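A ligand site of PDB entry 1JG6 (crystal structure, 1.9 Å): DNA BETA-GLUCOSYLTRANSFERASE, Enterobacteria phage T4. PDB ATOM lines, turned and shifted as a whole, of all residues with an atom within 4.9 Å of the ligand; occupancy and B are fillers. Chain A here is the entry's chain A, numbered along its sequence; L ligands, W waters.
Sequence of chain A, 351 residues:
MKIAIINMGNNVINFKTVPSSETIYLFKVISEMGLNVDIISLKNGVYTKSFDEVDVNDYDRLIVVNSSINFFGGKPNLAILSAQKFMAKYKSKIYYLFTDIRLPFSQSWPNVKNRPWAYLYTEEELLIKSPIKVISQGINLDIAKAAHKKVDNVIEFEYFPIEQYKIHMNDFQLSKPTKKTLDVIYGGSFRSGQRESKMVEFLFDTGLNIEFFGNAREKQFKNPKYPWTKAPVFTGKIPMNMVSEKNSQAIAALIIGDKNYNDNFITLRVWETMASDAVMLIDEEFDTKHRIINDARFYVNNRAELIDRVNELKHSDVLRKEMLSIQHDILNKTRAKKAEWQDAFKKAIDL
O of Gly 187 is in hydrogen-bond range of NH2 of Arg 269.
The backbone NH of Phe 213 lies within hydrogen-bond range of the backbone carbonyl oxygen of Tyr 186.
The backbone NH (N) of Arg 191 lies close to the side-chain hydroxyl (OG) of Ser 189 (3.2 Å).
The backbone carbonyl oxygen (O) of Ile 256 sits at hydrogen-bond distance from the guanidinium group (NH1) of Arg 195, at 3.3 Å.
The backbone NH (N) of Gly 214 sits at hydrogen-bond distance from the backbone carbonyl oxygen (O) of Gly 236, at 3.2 Å.
The guanidinium group (NH1) of Arg 195 lies within hydrogen-bond range of the side-chain hydroxyl (OH) of Tyr 186, 2.8 Å away.
OH of Tyr 186 sits at hydrogen-bond distance from NH2 of Arg 269 (3.2 Å).
N of Gly 188 lies within hydrogen-bond range of O of Phe 213 (2.9 Å).
Water W4 lies within hydrogen-bond range of O12 of the ligand (2.6 Å), N of Arg 269 (2.8 Å) and N of Leu 268 (3.4 Å).
Water W5 lies within hydrogen-bond range of OH of Tyr 261, O10 of the ligand and NH1 of Arg 191.
Water W6 lies within hydrogen-bond range of the side-chain hydroxyl of Thr 267 (2.6 Å), an oxygen (O11) of the ligand (2.8 Å) and the backbone carbonyl oxygen of Ile 256 (2.8 Å).
Water W2 lies within hydrogen-bond range of the side-chain hydroxyl of Tyr 186 (2.7 Å), the backbone carbonyl oxygen of Ser 189 (2.7 Å) and an oxygen (O7) of the ligand (2.9 Å).
Residues that only touch the ligand: Val 18, Gly 187, Gly 188, Phe 213, Gly 214, Lys 237, Pro 239, Val 243, Tyr 261 and Leu 268.
Hydrophobic or aromatic side chains that line the ligand: Val 18, Phe 213, Ile 238, Met 240, Val 243, Tyr 261 and Leu 268.
Within 4 Å of the ligand: Val 18, Gly 187, Gly 188, Ser 189, Arg 191, Arg 195, Phe 213, Gly 214, Lys 237, Ile 238, Pro 239, Met 240, Val 243, Tyr 261, Leu 268, Arg 269 and Glu 272.
The nearest printed residue that does not touch the ligand is Tyr 186 (4.2 Å).
The backbone carbonyl oxygen (O) of Ile 238 is in hydrogen-bond range of a nitrogen (N2) of the ligand (2.8 Å).
The guanidinium group (NH2) of Arg 195 lies within salt-bridge range of an oxygen (O10) of the ligand (2.8 Å).
O8 of the ligand is in salt-bridge range of NH1 of Arg 191 (2.8 Å).
The guanidinium group of Arg 269 is in salt-bridge range of an oxygen (O11) of the ligand.
The backbone NH (N) of Ile 238 lies within hydrogen-bond range of an oxygen (O2) of the ligand, 2.8 Å away.
The side-chain carboxylate of Glu 272 lies within hydrogen-bond range of an oxygen (O5) of the ligand.
The backbone NH (N) of Met 240 sits close to an oxygen (O1) of the ligand (3.4 Å).
The side-chain hydroxyl (OG) of Ser 189 lies within hydrogen-bond range of an oxygen (O7) of the ligand (3.5 Å).
An oxygen (O7) of the ligand sits at hydrogen-bond distance from the backbone NH (N) of Ser 189, 2.8 Å away.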
ATOM      1  N   VAL A  18      29.829  19.774  33.436  1.00  0.00           N
ATOM      2  CA  VAL A  18      29.992  18.850  32.322  1.00  0.00           C
ATOM      3  C   VAL A  18      31.387  18.890  31.701  1.00  0.00           C
ATOM      4  O   VAL A  18      32.014  17.837  31.515  1.00  0.00           O
ATOM      5  CB  VAL A  18      28.929  19.117  31.233  1.00  0.00           C
ATOM      6  CG1 VAL A  18      29.171  18.223  30.023  1.00  0.00           C
ATOM      7  CG2 VAL A  18      27.541  18.838  31.805  1.00  0.00           C
ATOM      8  N   ASP A 100      32.254  18.315  20.049  1.00  0.00           N
ATOM      9  CA  ASP A 100      31.108  19.213  19.857  1.00  0.00           C
ATOM     10  C   ASP A 100      31.326  20.059  18.611  1.00  0.00           C
ATOM     11  O   ASP A 100      32.283  20.815  18.531  1.00  0.00           O
ATOM     12  CB  ASP A 100      30.955  20.104  21.098  1.00  0.00           C
ATOM     13  CG  ASP A 100      29.638  20.847  21.120  1.00  0.00           C
ATOM     14  OD1 ASP A 100      29.060  20.971  22.227  1.00  0.00           O
ATOM     15  OD2 ASP A 100      29.175  21.319  20.055  1.00  0.00           O
ATOM     16  N   ARG A 102      30.136  22.738  17.553  1.00  0.00           N
ATOM     17  CA  ARG A 102      30.244  24.186  17.762  1.00  0.00           C
ATOM     18  C   ARG A 102      31.596  24.634  18.313  1.00  0.00           C
ATOM     19  O   ARG A 102      31.878  25.828  18.348  1.00  0.00           O
ATOM     20  CB  ARG A 102      29.167  24.655  18.743  1.00  0.00           C
ATOM     21  CG  ARG A 102      27.739  24.225  18.459  1.00  0.00           C
ATOM     22  CD  ARG A 102      26.899  24.493  19.693  1.00  0.00           C
ATOM     23  NE  ARG A 102      27.474  23.812  20.851  1.00  0.00           N
ATOM     24  CZ  ARG A 102      27.279  24.172  22.118  1.00  0.00           C
ATOM     25  NH1 ARG A 102      27.848  23.478  23.095  1.00  0.00           N
ATOM     26  NH2 ARG A 102      26.514  25.214  22.416  1.00  0.00           N
ATOM     27  N   TYR A 186      14.578  14.461  28.690  1.00  0.00           N
ATOM     28  CA  TYR A 186      15.706  14.884  27.871  1.00  0.00           C
ATOM     29  C   TYR A 186      16.564  15.817  28.713  1.00  0.00           C
ATOM     30  O   TYR A 186      16.066  16.777  29.299  1.00  0.00           O
ATOM     31  CB  TYR A 186      15.218  15.613  26.618  1.00  0.00           C
ATOM     32  CG  TYR A 186      16.327  16.196  25.756  1.00  0.00           C
ATOM     33  CD1 TYR A 186      16.855  17.467  26.037  1.00  0.00           C
ATOM     34  CD2 TYR A 186      16.841  15.494  24.660  1.00  0.00           C
ATOM     35  CE1 TYR A 186      17.878  18.012  25.247  1.00  0.00           C
ATOM     36  CE2 TYR A 186      17.855  16.033  23.861  1.00  0.00           C
ATOM     37  CZ  TYR A 186      18.368  17.300  24.161  1.00  0.00           C
ATOM     38  OH  TYR A 186      19.358  17.829  23.373  1.00  0.00           O
ATOM     39  N   GLY A 187      17.854  15.525  28.786  1.00  0.00           N
ATOM     40  CA  GLY A 187      18.756  16.358  29.557  1.00  0.00           C
ATOM     41  C   GLY A 187      19.808  16.993  28.673  1.00  0.00           C
ATOM     42  O   GLY A 187      20.443  16.308  27.873  1.00  0.00           O
ATOM     43  N   GLY A 188      19.980  18.308  28.825  1.00  0.00           N
ATOM     44  CA  GLY A 188      20.975  19.015  28.034  1.00  0.00           C
ATOM     45  C   GLY A 188      20.902  20.514  28.184  1.00  0.00           C
ATOM     46  O   GLY A 188      20.104  21.036  28.963  1.00  0.00           O
ATOM     47  N   SER A 189      21.736  21.224  27.426  1.00  0.00           N
ATOM     48  CA  SER A 189      21.749  22.683  27.465  1.00  0.00           C
ATOM     49  C   SER A 189      20.972  23.199  26.272  1.00  0.00           C
ATOM     50  O   SER A 189      20.525  22.425  25.427  1.00  0.00           O
ATOM     51  CB  SER A 189      23.184  23.222  27.434  1.00  0.00           C
ATOM     52  OG  SER A 189      23.771  23.054  26.151  1.00  0.00           O
ATOM     53  N   ARG A 191      22.231  24.805  23.973  1.00  0.00           N
ATOM     54  CA  ARG A 191      23.182  24.768  22.861  1.00  0.00           C
ATOM     55  C   ARG A 191      23.074  25.987  21.939  1.00  0.00           C
ATOM     56  O   ARG A 191      23.168  25.870  20.716  1.00  0.00           O
ATOM     57  CB  ARG A 191      22.991  23.499  22.039  1.00  0.00           C
ATOM     58  CG  ARG A 191      23.373  22.212  22.780  1.00  0.00           C
ATOM     59  CD  ARG A 191      23.259  21.019  21.867  1.00  0.00           C
ATOM     60  NE  ARG A 191      24.147  21.118  20.705  1.00  0.00           N
ATOM     61  CZ  ARG A 191      25.471  20.990  20.753  1.00  0.00           C
ATOM     62  NH1 ARG A 191      26.094  20.735  21.907  1.00  0.00           N
ATOM     63  NH2 ARG A 191      26.179  21.091  19.635  1.00  0.00           N
ATOM     64  N   ARG A 195      19.516  23.792  18.223  1.00  0.00           N
ATOM     65  CA  ARG A 195      18.625  22.634  18.154  1.00  0.00           C
ATOM     66  C   ARG A 195      17.211  22.994  18.608  1.00  0.00           C
ATOM     67  O   ARG A 195      16.447  22.125  19.007  1.00  0.00           O
ATOM     68  CB  ARG A 195      19.197  21.525  19.050  1.00  0.00           C
ATOM     69  CG  ARG A 195      18.617  20.142  18.846  1.00  0.00           C
ATOM     70  CD  ARG A 195      19.318  19.155  19.781  1.00  0.00           C
ATOM     71  NE  ARG A 195      20.755  19.049  19.495  1.00  0.00           N
ATOM     72  CZ  ARG A 195      21.608  18.340  20.233  1.00  0.00           C
ATOM     73  NH1 ARG A 195      21.185  17.664  21.305  1.00  0.00           N
ATOM     74  NH2 ARG A 195      22.889  18.283  19.885  1.00  0.00           N
ATOM     75  N   PHE A 213      15.736  18.369  31.767  1.00  0.00           N
ATOM     76  CA  PHE A 213      16.685  18.739  32.800  1.00  0.00           C
ATOM     77  C   PHE A 213      17.980  19.260  32.194  1.00  0.00           C
ATOM     78  O   PHE A 213      18.267  19.052  31.022  1.00  0.00           O
ATOM     79  CB  PHE A 213      16.968  17.563  33.767  1.00  0.00           C
ATOM     80  CG  PHE A 213      17.686  16.388  33.151  1.00  0.00           C
ATOM     81  CD1 PHE A 213      16.997  15.444  32.400  1.00  0.00           C
ATOM     82  CD2 PHE A 213      19.051  16.199  33.384  1.00  0.00           C
ATOM     83  CE1 PHE A 213      17.653  14.319  31.884  1.00  0.00           C
ATOM     84  CE2 PHE A 213      19.716  15.081  32.877  1.00  0.00           C
ATOM     85  CZ  PHE A 213      19.011  14.133  32.123  1.00  0.00           C
ATOM     86  N   GLY A 214      18.749  19.981  33.004  1.00  0.00           N
ATOM     87  CA  GLY A 214      19.997  20.544  32.524  1.00  0.00           C
ATOM     88  C   GLY A 214      20.003  22.051  32.559  1.00  0.00           C
ATOM     89  O   GLY A 214      19.190  22.675  33.249  1.00  0.00           O
ATOM     90  N   GLY A 236      16.623  21.720  37.288  1.00  0.00           N
ATOM     91  CA  GLY A 236      18.026  22.119  37.252  1.00  0.00           C
ATOM     92  C   GLY A 236      18.968  21.098  36.619  1.00  0.00           C
ATOM     93  O   GLY A 236      18.546  20.025  36.188  1.00  0.00           O
ATOM     94  N   LYS A 237      20.241  21.453  36.547  1.00  0.00           N
ATOM     95  CA  LYS A 237      21.237  20.548  35.982  1.00  0.00           C
ATOM     96  C   LYS A 237      21.652  19.559  37.057  1.00  0.00           C
ATOM     97  O   LYS A 237      21.480  19.808  38.249  1.00  0.00           O
ATOM     98  CB  LYS A 237      22.460  21.339  35.497  1.00  0.00           C
ATOM     99  CG  LYS A 237      23.239  22.009  36.608  1.00  0.00           C
ATOM    100  CD  LYS A 237      24.566  22.566  36.093  1.00  0.00           C
ATOM    101  CE  LYS A 237      25.413  23.143  37.230  1.00  0.00           C
ATOM    102  NZ  LYS A 237      26.761  23.563  36.764  1.00  0.00           N
ATOM    103  N   ILE A 238      22.207  18.427  36.645  1.00  0.00           N
ATOM    104  CA  ILE A 238      22.662  17.422  37.583  1.00  0.00           C
ATOM    105  C   ILE A 238      24.063  16.990  37.161  1.00  0.00           C
ATOM    106  O   ILE A 238      24.469  17.238  36.025  1.00  0.00           O
ATOM    107  CB  ILE A 238      21.734  16.190  37.606  1.00  0.00           C
ATOM    108  CG1 ILE A 238      21.758  15.494  36.240  1.00  0.00           C
ATOM    109  CG2 ILE A 238      20.310  16.614  37.967  1.00  0.00           C
ATOM    110  CD1 ILE A 238      20.959  14.208  36.219  1.00  0.00           C
ATOM    111  N   PRO A 239      24.818  16.371  38.068  1.00  0.00           N
ATOM    112  CA  PRO A 239      26.173  15.926  37.716  1.00  0.00           C
ATOM    113  C   PRO A 239      26.116  14.914  36.579  1.00  0.00           C
ATOM    114  O   PRO A 239      25.171  14.147  36.467  1.00  0.00           O
ATOM    115  CB  PRO A 239      26.696  15.312  39.011  1.00  0.00           C
ATOM    116  CG  PRO A 239      25.907  16.022  40.076  1.00  0.00           C
ATOM    117  CD  PRO A 239      24.528  16.075  39.481  1.00  0.00           C
ATOM    118  N   MET A 240      27.127  14.915  35.721  1.00  0.00           N
ATOM    119  CA  MET A 240      27.163  13.979  34.604  1.00  0.00           C
ATOM    120  C   MET A 240      27.085  12.524  35.072  1.00  0.00           C
ATOM    121  O   MET A 240      26.487  11.687  34.390  1.00  0.00           O
ATOM    122  CB  MET A 240      28.432  14.193  33.790  1.00  0.00           C
ATOM    123  CG  MET A 240      28.425  13.479  32.449  1.00  0.00           C
ATOM    124  SD  MET A 240      29.954  13.754  31.529  1.00  0.00           S
ATOM    125  CE  MET A 240      30.223  12.161  30.839  1.00  0.00           C
ATOM    126  N   VAL A 243      23.398  11.127  35.401  1.00  0.00           N
ATOM    127  CA  VAL A 243      22.523  11.221  34.230  1.00  0.00           C
ATOM    128  C   VAL A 243      21.684  10.001  33.893  1.00  0.00           C
ATOM    129  O   VAL A 243      20.479  10.119  33.652  1.00  0.00           O
ATOM    130  CB  VAL A 243      23.332  11.668  33.001  1.00  0.00           C
ATOM    131  CG1 VAL A 243      22.475  11.574  31.744  1.00  0.00           C
ATOM    132  CG2 VAL A 243      23.811  13.103  33.197  1.00  0.00           C
ATOM    133  N   ILE A 256      18.097  13.400  19.927  1.00  0.00           N
ATOM    134  CA  ILE A 256      18.054  14.377  18.839  1.00  0.00           C
ATOM    135  C   ILE A 256      19.438  15.022  18.813  1.00  0.00           C
ATOM    136  O   ILE A 256      20.203  14.870  19.764  1.00  0.00           O
ATOM    137  CB  ILE A 256      17.017  15.495  19.079  1.00  0.00           C
ATOM    138  CG1 ILE A 256      17.172  16.073  20.494  1.00  0.00           C
ATOM    139  CG2 ILE A 256      15.600  14.968  18.839  1.00  0.00           C
ATOM    140  CD1 ILE A 256      16.324  17.307  20.749  1.00  0.00           C
ATOM    141  N   TYR A 261      25.038  16.759  13.088  1.00  0.00           N
ATOM    142  CA  TYR A 261      25.257  15.512  13.817  1.00  0.00           C
ATOM    143  C   TYR A 261      24.556  14.370  13.090  1.00  0.00           C
ATOM    144  O   TYR A 261      24.943  13.216  13.224  1.00  0.00           O
ATOM    145  CB  TYR A 261      24.702  15.602  15.248  1.00  0.00           C
ATOM    146  CG  TYR A 261      25.576  16.351  16.235  1.00  0.00           C
ATOM    147  CD1 TYR A 261      26.814  16.860  15.850  1.00  0.00           C
ATOM    148  CD2 TYR A 261      25.159  16.531  17.557  1.00  0.00           C
ATOM    149  CE1 TYR A 261      27.621  17.545  16.770  1.00  0.00           C
ATOM    150  CE2 TYR A 261      25.956  17.210  18.469  1.00  0.00           C
ATOM    151  CZ  TYR A 261      27.185  17.713  18.075  1.00  0.00           C
ATOM    152  OH  TYR A 261      27.972  18.398  18.970  1.00  0.00           O
ATOM    153  N   THR A 267      26.326  10.634  19.935  1.00  0.00           N
ATOM    154  CA  THR A 267      26.614  11.434  21.109  1.00  0.00           C
ATOM    155  C   THR A 267      26.551  10.662  22.423  1.00  0.00           C
ATOM    156  O   THR A 267      26.084   9.527  22.478  1.00  0.00           O
ATOM    157  CB  THR A 267      25.643  12.625  21.191  1.00  0.00           C
ATOM    158  OG1 THR A 267      24.303  12.143  21.078  1.00  0.00           O
ATOM    159  CG2 THR A 267      25.925  13.614  20.064  1.00  0.00           C
ATOM    160  N   LEU A 268      27.053  11.297  23.490  1.00  0.00           N
ATOM    161  CA  LEU A 268      27.057  10.683  24.807  1.00  0.00           C
ATOM    162  C   LEU A 268      25.661  10.233  25.230  1.00  0.00           C
ATOM    163  O   LEU A 268      25.489   9.130  25.751  1.00  0.00           O
ATOM    164  CB  LEU A 268      27.589  11.676  25.857  1.00  0.00           C
ATOM    165  CG  LEU A 268      29.089  11.955  25.834  1.00  0.00           C
ATOM    166  CD1 LEU A 268      29.385  13.215  26.640  1.00  0.00           C
ATOM    167  CD2 LEU A 268      29.836  10.755  26.394  1.00  0.00           C
ATOM    168  N   ARG A 269      24.660  11.079  24.997  1.00  0.00           N
ATOM    169  CA  ARG A 269      23.292  10.752  25.374  1.00  0.00           C
ATOM    170  C   ARG A 269      22.806   9.448  24.757  1.00  0.00           C
ATOM    171  O   ARG A 269      21.931   8.789  25.315  1.00  0.00           O
ATOM    172  CB  ARG A 269      22.327  11.877  25.021  1.00  0.00           C
ATOM    173  CG  ARG A 269      22.044  12.045  23.534  1.00  0.00           C
ATOM    174  CD  ARG A 269      20.945  13.067  23.285  1.00  0.00           C
ATOM    175  NE  ARG A 269      21.313  14.416  23.732  1.00  0.00           N
ATOM    176  CZ  ARG A 269      20.998  14.931  24.915  1.00  0.00           C
ATOM    177  NH1 ARG A 269      20.300  14.224  25.800  1.00  0.00           N
ATOM    178  NH2 ARG A 269      21.386  16.162  25.215  1.00  0.00           N
ATOM    179  N   GLU A 272      24.172   7.074  27.295  1.00  0.00           N
ATOM    180  CA  GLU A 272      23.542   7.321  28.593  1.00  0.00           C
ATOM    181  C   GLU A 272      22.073   6.902  28.588  1.00  0.00           C
ATOM    182  O   GLU A 272      21.520   6.510  29.603  1.00  0.00           O
ATOM    183  CB  GLU A 272      23.626   8.809  28.962  1.00  0.00           C
ATOM    184  CG  GLU A 272      25.030   9.397  28.965  1.00  0.00           C
ATOM    185  CD  GLU A 272      25.025  10.904  29.163  1.00  0.00           C
ATOM    186  OE1 GLU A 272      24.141  11.578  28.588  1.00  0.00           O
ATOM    187  OE2 GLU A 272      25.902  11.413  29.899  1.00  0.00           O
HETATM  188  N1  LIG L   1      24.370  16.648  31.065  1.00  0.00           N
HETATM  189  C1  LIG L   1      24.723  16.595  32.406  1.00  0.00           C
HETATM  190  N2  LIG L   1      23.802  17.122  33.270  1.00  0.00           N
HETATM  191  C2  LIG L   1      22.584  17.702  32.939  1.00  0.00           C
HETATM  192  C3  LIG L   1      22.284  17.706  31.539  1.00  0.00           C
HETATM  193  C4  LIG L   1      23.173  17.196  30.675  1.00  0.00           C
HETATM  194  O1  LIG L   1      25.762  16.107  32.797  1.00  0.00           O
HETATM  195  O2  LIG L   1      21.889  18.177  33.835  1.00  0.00           O
HETATM  196  C5  LIG L   1      25.337  16.112  30.088  1.00  0.00           C
HETATM  197  C6  LIG L   1      25.085  14.668  29.663  1.00  0.00           C
HETATM  198  O3  LIG L   1      26.305  13.967  29.590  1.00  0.00           O
HETATM  199  C7  LIG L   1      24.397  14.851  28.305  1.00  0.00           C
HETATM  200  C8  LIG L   1      25.095  16.087  27.755  1.00  0.00           C
HETATM  201  O4  LIG L   1      25.289  16.925  28.923  1.00  0.00           O
HETATM  202  O5  LIG L   1      24.583  13.749  27.431  1.00  0.00           O
HETATM  203  C9  LIG L   1      24.309  16.840  26.718  1.00  0.00           C
HETATM  204  O6  LIG L   1      25.116  17.841  26.110  1.00  0.00           O
HETATM  205  P1  LIG L   1      24.471  18.881  25.089  1.00  0.00           P
HETATM  206  O7  LIG L   1      23.377  19.605  25.805  1.00  0.00           O
HETATM  207  O8  LIG L   1      25.566  19.654  24.443  1.00  0.00           O
HETATM  208  O9  LIG L   1      23.758  17.949  24.007  1.00  0.00           O
HETATM  209  P2  LIG L   1      24.370  16.913  22.958  1.00  0.00           P
HETATM  210  O10 LIG L   1      24.830  17.830  21.884  1.00  0.00           O
HETATM  211  O11 LIG L   1      23.153  16.114  22.644  1.00  0.00           O
HETATM  212  O12 LIG L   1      25.422  16.234  23.746  1.00  0.00           O
HETATM  213  O   HOH W   1      28.071  16.223  24.527  1.00  0.00           O
HETATM  214  O   HOH W   2      20.818  19.871  24.470  1.00  0.00           O
HETATM  215  O   HOH W   3      23.076  21.029  30.916  1.00  0.00           O
HETATM  216  O   HOH W   4      25.071  13.798  24.679  1.00  0.00           O
HETATM  217  O   HOH W   5      27.494  17.880  21.415  1.00  0.00           O
HETATM  218  O   HOH W   6      22.818  14.267  20.569  1.00  0.00           O
HETATM  219  O   HOH W   7      24.694  19.678  28.761  1.00  0.00           O
